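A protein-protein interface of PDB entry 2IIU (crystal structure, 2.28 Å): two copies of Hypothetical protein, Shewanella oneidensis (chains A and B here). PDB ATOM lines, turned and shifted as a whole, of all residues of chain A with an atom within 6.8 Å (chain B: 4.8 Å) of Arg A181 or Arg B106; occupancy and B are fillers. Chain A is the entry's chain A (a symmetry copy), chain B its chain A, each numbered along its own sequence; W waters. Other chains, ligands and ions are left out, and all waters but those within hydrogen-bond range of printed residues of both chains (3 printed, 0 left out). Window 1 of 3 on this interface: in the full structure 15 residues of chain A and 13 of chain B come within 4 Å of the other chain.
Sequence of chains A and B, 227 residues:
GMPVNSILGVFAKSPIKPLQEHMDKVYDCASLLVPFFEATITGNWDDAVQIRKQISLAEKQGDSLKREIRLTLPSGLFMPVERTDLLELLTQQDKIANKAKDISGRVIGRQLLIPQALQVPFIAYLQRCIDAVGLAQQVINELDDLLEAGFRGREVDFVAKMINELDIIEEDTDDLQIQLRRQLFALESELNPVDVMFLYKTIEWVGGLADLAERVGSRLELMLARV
Position printed for both chains: 205.
Of the 7 pairs that touch across the chains among the printed residues, none has its exchanged pair printed and touching as well.
The side-chain carboxylate (OE2) of Glu A188 lies within hydrogen-bond range of the side-chain hydroxyl (OH) of Tyr A200 (2.5 Å).
The side-chain amide nitrogen (NE2) of Gln A177 sits close to the guanidinium group (NH1) of Arg A181 (3.4 Å).
The side-chain hydroxyl of Tyr A200 sits at hydrogen-bond distance from the guanidinium group of Arg B110, at 3.3 Å.
The side-chain carboxylate (OE2) of Glu A188 lies within salt-bridge range of the guanidinium group (NH1) of Arg B110, at 2.8 Å.
Water W2 lies within hydrogen-bond range of the backbone carbonyl oxygen of Tyr A200 (2.5 Å), the guanidinium group of Arg A181 (3.0 Å) and the guanidinium group of Arg B106 (3.3 Å).
Water W3 lies within hydrogen-bond range of the guanidinium group of Arg B106 (2.7 Å), the side-chain hydroxyl of Tyr A200 (3.2 Å) and the guanidinium group of Arg B110 (3.3 Å).
Water W1 bridges the indole nitrogen (NE1) of Trp B205 (3.3 Å) and the side-chain carboxylate (OE2) of Glu A204 (3.5 Å).
Of the 11 printed residues of chain B, 4 touch a printed residue of chain A.
Printed residues of chain A that touch a printed residue of chain B: Arg A181, Phe A185, Glu A188 and Tyr A200.
Along chain A the printed residues that touch a printed residue of chain B span positions 181 to 200.
Among the printed residues, 7 pairs touch across the chains.
Arg A181 touches Arg B106 (CD to NH1, 3.7 Å).
O of Gly B109 touches CE2 of Phe A185 (3.9 Å).
Arg B110 touches Phe A185 (NH1 to CD1, 3.5 Å).
Tyr A200 touches Arg B106.
CD2 of Tyr A200 touches CZ of Phe B198, at 3.7 Å.
Printed residues of chain B within 4 Å of Phe A185: Gly B109 (3.9 Å) and Arg B110 (3.5 Å).
Ala A186 touches none of the printed residues of chain B.
Of the printed residues of chain B, Glu A188 touches Arg B110 (2.8 Å).
Printed residues of chain A within 4 Å of Arg B106: Arg A181 and Tyr A200.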
ATOM      1  N   LEU A 118      16.107  25.483  -7.814  1.00  0.00           N
ATOM      2  CA  LEU A 118      17.459  24.962  -7.893  1.00  0.00           C
ATOM      3  C   LEU A 118      17.953  24.392  -6.573  1.00  0.00           C
ATOM      4  O   LEU A 118      19.011  23.780  -6.542  1.00  0.00           O
ATOM      5  CB  LEU A 118      18.406  26.099  -8.258  1.00  0.00           C
ATOM      6  CG  LEU A 118      18.206  26.850  -9.584  1.00  0.00           C
ATOM      7  CD1 LEU A 118      19.387  27.750  -9.805  1.00  0.00           C
ATOM      8  CD2 LEU A 118      18.092  25.901 -10.730  1.00  0.00           C
ATOM      9  N   TYR A 125      24.086  18.148  -6.096  1.00  0.00           N
ATOM     10  CA  TYR A 125      25.338  18.405  -6.834  1.00  0.00           C
ATOM     11  C   TYR A 125      26.519  18.693  -5.872  1.00  0.00           C
ATOM     12  O   TYR A 125      27.625  18.142  -6.015  1.00  0.00           O
ATOM     13  CB  TYR A 125      25.137  19.576  -7.807  1.00  0.00           C
ATOM     14  CG  TYR A 125      26.404  20.111  -8.488  1.00  0.00           C
ATOM     15  CD1 TYR A 125      27.116  19.332  -9.406  1.00  0.00           C
ATOM     16  CD2 TYR A 125      26.836  21.417  -8.271  1.00  0.00           C
ATOM     17  CE1 TYR A 125      28.273  19.828 -10.038  1.00  0.00           C
ATOM     18  CE2 TYR A 125      27.996  21.913  -8.901  1.00  0.00           C
ATOM     19  CZ  TYR A 125      28.690  21.112  -9.778  1.00  0.00           C
ATOM     20  OH  TYR A 125      29.784  21.611 -10.418  1.00  0.00           O
ATOM     21  N   LEU A 176      24.559  15.882 -13.018  1.00  0.00           N
ATOM     22  CA  LEU A 176      23.919  16.827 -12.115  1.00  0.00           C
ATOM     23  C   LEU A 176      24.241  18.268 -12.466  1.00  0.00           C
ATOM     24  O   LEU A 176      23.386  19.128 -12.381  1.00  0.00           O
ATOM     25  CB  LEU A 176      24.306  16.519 -10.667  1.00  0.00           C
ATOM     26  CG  LEU A 176      23.838  15.180 -10.099  1.00  0.00           C
ATOM     27  CD1 LEU A 176      24.413  15.002  -8.705  1.00  0.00           C
ATOM     28  CD2 LEU A 176      22.339  15.093 -10.049  1.00  0.00           C
ATOM     29  N   GLN A 177      25.465  18.515 -12.905  1.00  0.00           N
ATOM     30  CA  GLN A 177      25.905  19.856 -13.274  1.00  0.00           C
ATOM     31  C   GLN A 177      25.129  20.355 -14.472  1.00  0.00           C
ATOM     32  O   GLN A 177      24.698  21.508 -14.519  1.00  0.00           O
ATOM     33  CB  GLN A 177      27.393  19.838 -13.622  1.00  0.00           C
ATOM     34  CG  GLN A 177      28.004  21.224 -13.673  1.00  0.00           C
ATOM     35  CD  GLN A 177      29.517  21.177 -13.858  1.00  0.00           C
ATOM     36  OE1 GLN A 177      30.271  21.731 -13.042  1.00  0.00           O
ATOM     37  NE2 GLN A 177      29.963  20.457 -14.870  1.00  0.00           N
ATOM     38  N   ILE A 178      24.908  19.455 -15.433  1.00  0.00           N
ATOM     39  CA  ILE A 178      24.156  19.793 -16.625  1.00  0.00           C
ATOM     40  C   ILE A 178      22.704  20.128 -16.298  1.00  0.00           C
ATOM     41  O   ILE A 178      22.190  21.148 -16.781  1.00  0.00           O
ATOM     42  CB  ILE A 178      24.250  18.682 -17.664  1.00  0.00           C
ATOM     43  CG1 ILE A 178      25.685  18.630 -18.198  1.00  0.00           C
ATOM     44  CG2 ILE A 178      23.239  18.938 -18.803  1.00  0.00           C
ATOM     45  CD1 ILE A 178      25.979  17.403 -19.119  1.00  0.00           C
ATOM     46  N   GLN A 179      22.050  19.273 -15.513  1.00  0.00           N
ATOM     47  CA  GLN A 179      20.676  19.513 -15.094  1.00  0.00           C
ATOM     48  C   GLN A 179      20.572  20.833 -14.338  1.00  0.00           C
ATOM     49  O   GLN A 179      19.718  21.643 -14.606  1.00  0.00           O
ATOM     50  CB  GLN A 179      20.171  18.382 -14.206  1.00  0.00           C
ATOM     51  CG  GLN A 179      19.981  17.018 -14.900  1.00  0.00           C
ATOM     52  N   LEU A 180      21.512  21.086 -13.450  1.00  0.00           N
ATOM     53  CA  LEU A 180      21.496  22.309 -12.677  1.00  0.00           C
ATOM     54  C   LEU A 180      21.623  23.566 -13.580  1.00  0.00           C
ATOM     55  O   LEU A 180      20.889  24.530 -13.409  1.00  0.00           O
ATOM     56  CB  LEU A 180      22.605  22.211 -11.644  1.00  0.00           C
ATOM     57  CG  LEU A 180      22.749  23.277 -10.594  1.00  0.00           C
ATOM     58  CD1 LEU A 180      21.470  23.363  -9.761  1.00  0.00           C
ATOM     59  CD2 LEU A 180      23.948  22.858  -9.750  1.00  0.00           C
ATOM     60  N   ARG A 181      22.536  23.543 -14.541  1.00  0.00           N
ATOM     61  CA  ARG A 181      22.678  24.661 -15.496  1.00  0.00           C
ATOM     62  C   ARG A 181      21.489  24.827 -16.420  1.00  0.00           C
ATOM     63  O   ARG A 181      21.175  25.932 -16.829  1.00  0.00           O
ATOM     64  CB  ARG A 181      23.921  24.489 -16.337  1.00  0.00           C
ATOM     65  CG  ARG A 181      25.155  24.684 -15.524  1.00  0.00           C
ATOM     66  CD  ARG A 181      26.440  24.615 -16.368  1.00  0.00           C
ATOM     67  NE  ARG A 181      27.542  24.944 -15.479  1.00  0.00           N
ATOM     68  CZ  ARG A 181      28.731  24.340 -15.487  1.00  0.00           C
ATOM     69  NH1 ARG A 181      28.982  23.346 -16.337  1.00  0.00           N
ATOM     70  NH2 ARG A 181      29.664  24.709 -14.607  1.00  0.00           N
ATOM     71  N   ARG A 182      20.875  23.714 -16.796  1.00  0.00           N
ATOM     72  CA  ARG A 182      19.689  23.724 -17.649  1.00  0.00           C
ATOM     73  C   ARG A 182      18.573  24.462 -16.875  1.00  0.00           C
ATOM     74  O   ARG A 182      17.858  25.285 -17.422  1.00  0.00           O
ATOM     75  CB  ARG A 182      19.279  22.275 -17.960  1.00  0.00           C
ATOM     76  CG  ARG A 182      18.097  22.080 -18.933  1.00  0.00           C
ATOM     77  CD  ARG A 182      17.935  20.562 -19.329  1.00  0.00           C
ATOM     78  NE  ARG A 182      19.202  19.927 -19.764  1.00  0.00           N
ATOM     79  CZ  ARG A 182      19.378  18.617 -19.968  1.00  0.00           C
ATOM     80  N   GLN A 183      18.435  24.158 -15.595  1.00  0.00           N
ATOM     81  CA  GLN A 183      17.436  24.825 -14.788  1.00  0.00           C
ATOM     82  C   GLN A 183      17.709  26.287 -14.608  1.00  0.00           C
ATOM     83  O   GLN A 183      16.787  27.082 -14.575  1.00  0.00           O
ATOM     84  CB  GLN A 183      17.341  24.204 -13.396  1.00  0.00           C
ATOM     85  CG  GLN A 183      16.601  22.882 -13.386  1.00  0.00           C
ATOM     86  CD  GLN A 183      16.560  22.231 -12.018  1.00  0.00           C
ATOM     87  OE1 GLN A 183      17.488  22.382 -11.215  1.00  0.00           O
ATOM     88  NE2 GLN A 183      15.508  21.473 -11.761  1.00  0.00           N
ATOM     89  N   LEU A 184      18.974  26.638 -14.418  1.00  0.00           N
ATOM     90  CA  LEU A 184      19.318  28.043 -14.256  1.00  0.00           C
ATOM     91  C   LEU A 184      19.018  28.774 -15.547  1.00  0.00           C
ATOM     92  O   LEU A 184      18.436  29.828 -15.522  1.00  0.00           O
ATOM     93  CB  LEU A 184      20.790  28.194 -13.812  1.00  0.00           C
ATOM     94  CG  LEU A 184      21.330  29.601 -13.524  1.00  0.00           C
ATOM     95  CD1 LEU A 184      20.390  30.445 -12.700  1.00  0.00           C
ATOM     96  CD2 LEU A 184      22.645  29.546 -12.889  1.00  0.00           C
ATOM     97  N   PHE A 185      19.369  28.178 -16.678  1.00  0.00           N
ATOM     98  CA  PHE A 185      19.133  28.768 -17.990  1.00  0.00           C
ATOM     99  C   PHE A 185      17.654  29.160 -18.170  1.00  0.00           C
ATOM    100  O   PHE A 185      17.334  30.265 -18.656  1.00  0.00           O
ATOM    101  CB  PHE A 185      19.602  27.809 -19.065  1.00  0.00           C
ATOM    102  CG  PHE A 185      19.530  28.370 -20.438  1.00  0.00           C
ATOM    103  CD1 PHE A 185      20.254  29.484 -20.778  1.00  0.00           C
ATOM    104  CD2 PHE A 185      18.757  27.765 -21.411  1.00  0.00           C
ATOM    105  CE1 PHE A 185      20.194  30.010 -22.062  1.00  0.00           C
ATOM    106  CE2 PHE A 185      18.702  28.284 -22.693  1.00  0.00           C
ATOM    107  CZ  PHE A 185      19.419  29.416 -23.017  1.00  0.00           C
ATOM    108  N   ALA A 186      16.753  28.280 -17.725  1.00  0.00           N
ATOM    109  CA  ALA A 186      15.312  28.540 -17.794  1.00  0.00           C
ATOM    110  C   ALA A 186      14.861  29.687 -16.905  1.00  0.00           C
ATOM    111  O   ALA A 186      13.852  30.318 -17.185  1.00  0.00           O
ATOM    112  CB  ALA A 186      14.545  27.288 -17.390  1.00  0.00           C
ATOM    113  N   GLU A 188      16.876  32.407 -16.059  1.00  0.00           N
ATOM    114  CA  GLU A 188      17.635  33.651 -16.260  1.00  0.00           C
ATOM    115  C   GLU A 188      16.752  34.873 -16.509  1.00  0.00           C
ATOM    116  O   GLU A 188      17.055  35.948 -15.974  1.00  0.00           O
ATOM    117  CB  GLU A 188      18.665  33.501 -17.368  1.00  0.00           C
ATOM    118  CG  GLU A 188      19.747  32.459 -17.023  1.00  0.00           C
ATOM    119  CD  GLU A 188      20.759  32.303 -18.138  1.00  0.00           C
ATOM    120  OE1 GLU A 188      20.705  33.131 -19.088  1.00  0.00           O
ATOM    121  OE2 GLU A 188      21.602  31.359 -18.064  1.00  0.00           O
ATOM    122  N   TYR A 200      26.145  30.952 -11.689  1.00  0.00           N
ATOM    123  CA  TYR A 200      27.042  30.145 -12.496  1.00  0.00           C
ATOM    124  C   TYR A 200      28.395  30.017 -11.850  1.00  0.00           C
ATOM    125  O   TYR A 200      28.962  28.948 -11.885  1.00  0.00           O
ATOM    126  CB  TYR A 200      27.204  30.714 -13.922  1.00  0.00           C
ATOM    127  CG  TYR A 200      26.015  30.377 -14.785  1.00  0.00           C
ATOM    128  CD1 TYR A 200      25.795  29.074 -15.181  1.00  0.00           C
ATOM    129  CD2 TYR A 200      25.099  31.356 -15.191  1.00  0.00           C
ATOM    130  CE1 TYR A 200      24.678  28.729 -15.975  1.00  0.00           C
ATOM    131  CE2 TYR A 200      24.028  31.027 -15.994  1.00  0.00           C
ATOM    132  CZ  TYR A 200      23.826  29.703 -16.377  1.00  0.00           C
ATOM    133  OH  TYR A 200      22.752  29.363 -17.143  1.00  0.00           O
ATOM    134  N   LYS A 201      28.965  31.104 -11.330  1.00  0.00           N
ATOM    135  CA  LYS A 201      30.284  31.029 -10.648  1.00  0.00           C
ATOM    136  C   LYS A 201      30.253  30.086  -9.457  1.00  0.00           C
ATOM    137  O   LYS A 201      31.199  29.368  -9.220  1.00  0.00           O
ATOM    138  CB  LYS A 201      30.787  32.392 -10.144  1.00  0.00           C
ATOM    139  CG  LYS A 201      31.579  33.217 -11.171  1.00  0.00           C
ATOM    140  CD  LYS A 201      31.630  34.732 -10.802  1.00  0.00           C
ATOM    141  N   ILE A 203      28.271  27.411  -9.057  1.00  0.00           N
ATOM    142  CA  ILE A 203      28.236  26.049  -9.569  1.00  0.00           C
ATOM    143  C   ILE A 203      29.651  25.640  -9.996  1.00  0.00           C
ATOM    144  O   ILE A 203      30.084  24.555  -9.697  1.00  0.00           O
ATOM    145  CB  ILE A 203      27.265  25.980 -10.717  1.00  0.00           C
ATOM    146  CG1 ILE A 203      25.861  26.232 -10.168  1.00  0.00           C
ATOM    147  CG2 ILE A 203      27.337  24.634 -11.452  1.00  0.00           C
ATOM    148  CD1 ILE A 203      24.826  26.417 -11.212  1.00  0.00           C
ATOM    149  N   GLU A 204      30.356  26.537 -10.682  1.00  0.00           N
ATOM    150  CA  GLU A 204      31.706  26.307 -11.121  1.00  0.00           C
ATOM    151  C   GLU A 204      32.641  26.037  -9.959  1.00  0.00           C
ATOM    152  O   GLU A 204      33.416  25.085 -10.000  1.00  0.00           O
ATOM    153  CB  GLU A 204      32.205  27.536 -11.899  1.00  0.00           C
ATOM    154  CG  GLU A 204      33.642  27.450 -12.398  1.00  0.00           C
ATOM    155  CD  GLU A 204      34.284  28.824 -12.788  1.00  0.00           C
ATOM    156  OE1 GLU A 204      33.607  29.883 -12.822  1.00  0.00           O
ATOM    157  OE2 GLU A 204      35.505  28.833 -13.054  1.00  0.00           O
ATOM    158  N   TRP A 205      32.602  26.901  -8.942  1.00  0.00           N
ATOM    159  CA  TRP A 205      33.425  26.751  -7.772  1.00  0.00           C
ATOM    160  C   TRP A 205      33.188  25.433  -7.056  1.00  0.00           C
ATOM    161  O   TRP A 205      34.135  24.798  -6.640  1.00  0.00           O
ATOM    162  CB  TRP A 205      33.234  27.868  -6.757  1.00  0.00           C
ATOM    163  CG  TRP A 205      33.716  29.211  -7.181  1.00  0.00           C
ATOM    164  CD1 TRP A 205      34.779  29.500  -8.013  1.00  0.00           C
ATOM    165  CD2 TRP A 205      33.177  30.477  -6.770  1.00  0.00           C
ATOM    166  NE1 TRP A 205      34.911  30.861  -8.147  1.00  0.00           N
ATOM    167  CE2 TRP A 205      33.950  31.483  -7.390  1.00  0.00           C
ATOM    168  CE3 TRP A 205      32.120  30.858  -5.927  1.00  0.00           C
ATOM    169  CZ2 TRP A 205      33.699  32.842  -7.192  1.00  0.00           C
ATOM    170  CZ3 TRP A 205      31.864  32.210  -5.742  1.00  0.00           C
ATOM    171  CH2 TRP A 205      32.660  33.188  -6.376  1.00  0.00           C
ATOM    172  N   ASP B 102      33.774  20.099 -23.042  1.00  0.00           N
ATOM    173  CA  ASP B 102      33.114  21.086 -22.217  1.00  0.00           C
ATOM    174  C   ASP B 102      32.577  22.290 -23.016  1.00  0.00           C
ATOM    175  O   ASP B 102      31.458  22.730 -22.810  1.00  0.00           O
ATOM    176  CB  ASP B 102      34.081  21.623 -21.118  1.00  0.00           C
ATOM    177  CG  ASP B 102      34.264  20.632 -19.953  1.00  0.00           C
ATOM    178  OD1 ASP B 102      33.583  19.578 -19.911  1.00  0.00           O
ATOM    179  OD2 ASP B 102      35.101  20.907 -19.071  1.00  0.00           O
ATOM    180  N   ILE B 103      33.415  22.867 -23.859  1.00  0.00           N
ATOM    181  CA  ILE B 103      33.012  23.989 -24.670  1.00  0.00           C
ATOM    182  C   ILE B 103      31.794  23.618 -25.538  1.00  0.00           C
ATOM    183  O   ILE B 103      30.807  24.341 -25.581  1.00  0.00           O
ATOM    184  CB  ILE B 103      34.139  24.410 -25.621  1.00  0.00           C
ATOM    185  CG1 ILE B 103      35.313  24.973 -24.818  1.00  0.00           C
ATOM    186  CG2 ILE B 103      33.597  25.433 -26.670  1.00  0.00           C
ATOM    187  CD1 ILE B 103      36.509  25.375 -25.620  1.00  0.00           C
ATOM    188  N   SER B 104      31.881  22.499 -26.241  1.00  0.00           N
ATOM    189  CA  SER B 104      30.787  22.102 -27.110  1.00  0.00           C
ATOM    190  C   SER B 104      29.484  21.883 -26.354  1.00  0.00           C
ATOM    191  O   SER B 104      28.417  22.257 -26.853  1.00  0.00           O
ATOM    192  CB  SER B 104      31.149  20.843 -27.934  1.00  0.00           C
ATOM    193  OG  SER B 104      31.629  19.801 -27.095  1.00  0.00           O
ATOM    194  N   GLY B 105      29.570  21.295 -25.161  1.00  0.00           N
ATOM    195  CA  GLY B 105      28.393  21.066 -24.314  1.00  0.00           C
ATOM    196  C   GLY B 105      27.762  22.357 -23.873  1.00  0.00           C
ATOM    197  O   GLY B 105      26.560  22.490 -23.942  1.00  0.00           O
ATOM    198  N   ARG B 106      28.570  23.325 -23.414  1.00  0.00           N
ATOM    199  CA  ARG B 106      28.024  24.601 -22.951  1.00  0.00           C
ATOM    200  C   ARG B 106      27.336  25.349 -24.107  1.00  0.00           C
ATOM    201  O   ARG B 106      26.264  25.969 -23.951  1.00  0.00           O
ATOM    202  CB  ARG B 106      29.131  25.401 -22.218  1.00  0.00           C
ATOM    203  CG  ARG B 106      29.438  24.801 -20.748  1.00  0.00           C
ATOM    204  CD  ARG B 106      28.450  25.371 -19.670  1.00  0.00           C
ATOM    205  NE  ARG B 106      29.060  26.338 -18.705  1.00  0.00           N
ATOM    206  CZ  ARG B 106      28.399  27.340 -18.144  1.00  0.00           C
ATOM    207  NH1 ARG B 106      27.131  27.544 -18.485  1.00  0.00           N
ATOM    208  NH2 ARG B 106      28.996  28.180 -17.247  1.00  0.00           N
ATOM    209  N   VAL B 107      27.906  25.242 -25.299  1.00  0.00           N
ATOM    210  CA  VAL B 107      27.355  25.928 -26.470  1.00  0.00           C
ATOM    211  C   VAL B 107      26.004  25.301 -26.875  1.00  0.00           C
ATOM    212  O   VAL B 107      25.029  25.985 -27.145  1.00  0.00           O
ATOM    213  CB  VAL B 107      28.384  25.919 -27.612  1.00  0.00           C
ATOM    214  CG1 VAL B 107      27.763  26.380 -28.912  1.00  0.00           C
ATOM    215  CG2 VAL B 107      29.540  26.834 -27.235  1.00  0.00           C
ATOM    216  N   ILE B 108      25.948  23.989 -26.914  1.00  0.00           N
ATOM    217  CA  ILE B 108      24.669  23.317 -27.171  1.00  0.00           C
ATOM    218  C   ILE B 108      23.642  23.642 -26.084  1.00  0.00           C
ATOM    219  O   ILE B 108      22.490  23.908 -26.372  1.00  0.00           O
ATOM    220  CB  ILE B 108      24.858  21.791 -27.245  1.00  0.00           C
ATOM    221  CG1 ILE B 108      25.596  21.441 -28.517  1.00  0.00           C
ATOM    222  CG2 ILE B 108      23.523  21.072 -27.208  1.00  0.00           C
ATOM    223  CD1 ILE B 108      24.856  21.725 -29.818  1.00  0.00           C
ATOM    224  N   GLY B 109      24.069  23.640 -24.836  1.00  0.00           N
ATOM    225  CA  GLY B 109      23.162  23.926 -23.735  1.00  0.00           C
ATOM    226  C   GLY B 109      22.520  25.319 -23.758  1.00  0.00           C
ATOM    227  O   GLY B 109      21.401  25.469 -23.295  1.00  0.00           O
ATOM    228  N   ARG B 110      23.213  26.341 -24.260  1.00  0.00           N
ATOM    229  CA  ARG B 110      22.617  27.655 -24.322  1.00  0.00           C
ATOM    230  C   ARG B 110      22.143  27.979 -25.715  1.00  0.00           C
ATOM    231  O   ARG B 110      21.547  29.019 -25.902  1.00  0.00           O
ATOM    232  CB  ARG B 110      23.646  28.719 -23.944  1.00  0.00           C
ATOM    233  CG  ARG B 110      24.216  28.606 -22.556  1.00  0.00           C
ATOM    234  CD  ARG B 110      24.995  29.861 -22.176  1.00  0.00           C
ATOM    235  NE  ARG B 110      24.192  31.077 -22.166  1.00  0.00           N
ATOM    236  CZ  ARG B 110      23.479  31.501 -21.140  1.00  0.00           C
ATOM    237  NH1 ARG B 110      23.442  30.793 -20.045  1.00  0.00           N
ATOM    238  NH2 ARG B 110      22.771  32.617 -21.233  1.00  0.00           N
ATOM    239  N   PHE B 198      28.752  35.280 -21.591  1.00  0.00           N
ATOM    240  CA  PHE B 198      29.030  33.942 -22.100  1.00  0.00           C
ATOM    241  C   PHE B 198      29.825  33.942 -23.403  1.00  0.00           C
ATOM    242  O   PHE B 198      30.448  32.930 -23.756  1.00  0.00           O
ATOM    243  CB  PHE B 198      27.774  33.065 -22.147  1.00  0.00           C
ATOM    244  CG  PHE B 198      27.479  32.413 -20.830  1.00  0.00           C
ATOM    245  CD1 PHE B 198      28.183  31.277 -20.440  1.00  0.00           C
ATOM    246  CD2 PHE B 198      26.556  32.957 -19.943  1.00  0.00           C
ATOM    247  CE1 PHE B 198      27.941  30.700 -19.192  1.00  0.00           C
ATOM    248  CE2 PHE B 198      26.316  32.398 -18.733  1.00  0.00           C
ATOM    249  CZ  PHE B 198      27.018  31.271 -18.343  1.00  0.00           C
ATOM    250  N   TRP B 205      37.711  30.333 -23.083  1.00  0.00           N
ATOM    251  CA  TRP B 205      37.829  28.901 -23.155  1.00  0.00           C
ATOM    252  C   TRP B 205      38.574  28.436 -24.392  1.00  0.00           C
ATOM    253  O   TRP B 205      39.396  27.548 -24.300  1.00  0.00           O
ATOM    254  CB  TRP B 205      36.486  28.188 -23.130  1.00  0.00           C
ATOM    255  CG  TRP B 205      35.735  28.274 -21.846  1.00  0.00           C
ATOM    256  CD1 TRP B 205      36.257  28.352 -20.571  1.00  0.00           C
ATOM    257  CD2 TRP B 205      34.308  28.257 -21.693  1.00  0.00           C
ATOM    258  NE1 TRP B 205      35.236  28.400 -19.652  1.00  0.00           N
ATOM    259  CE2 TRP B 205      34.034  28.333 -20.310  1.00  0.00           C
ATOM    260  CE3 TRP B 205      33.232  28.171 -22.593  1.00  0.00           C
ATOM    261  CZ2 TRP B 205      32.731  28.327 -19.807  1.00  0.00           C
ATOM    262  CZ3 TRP B 205      31.937  28.179 -22.092  1.00  0.00           C
ATOM    263  CH2 TRP B 205      31.702  28.254 -20.703  1.00  0.00           C
HETATM  264  O   HOH W   1      36.019  28.466 -16.473  1.00  0.00           O
HETATM  265  O   HOH W   2      28.740  27.536 -13.972  1.00  0.00           O
HETATM  266  O   HOH W   3      24.532  27.807 -19.265  1.00  0.00           O
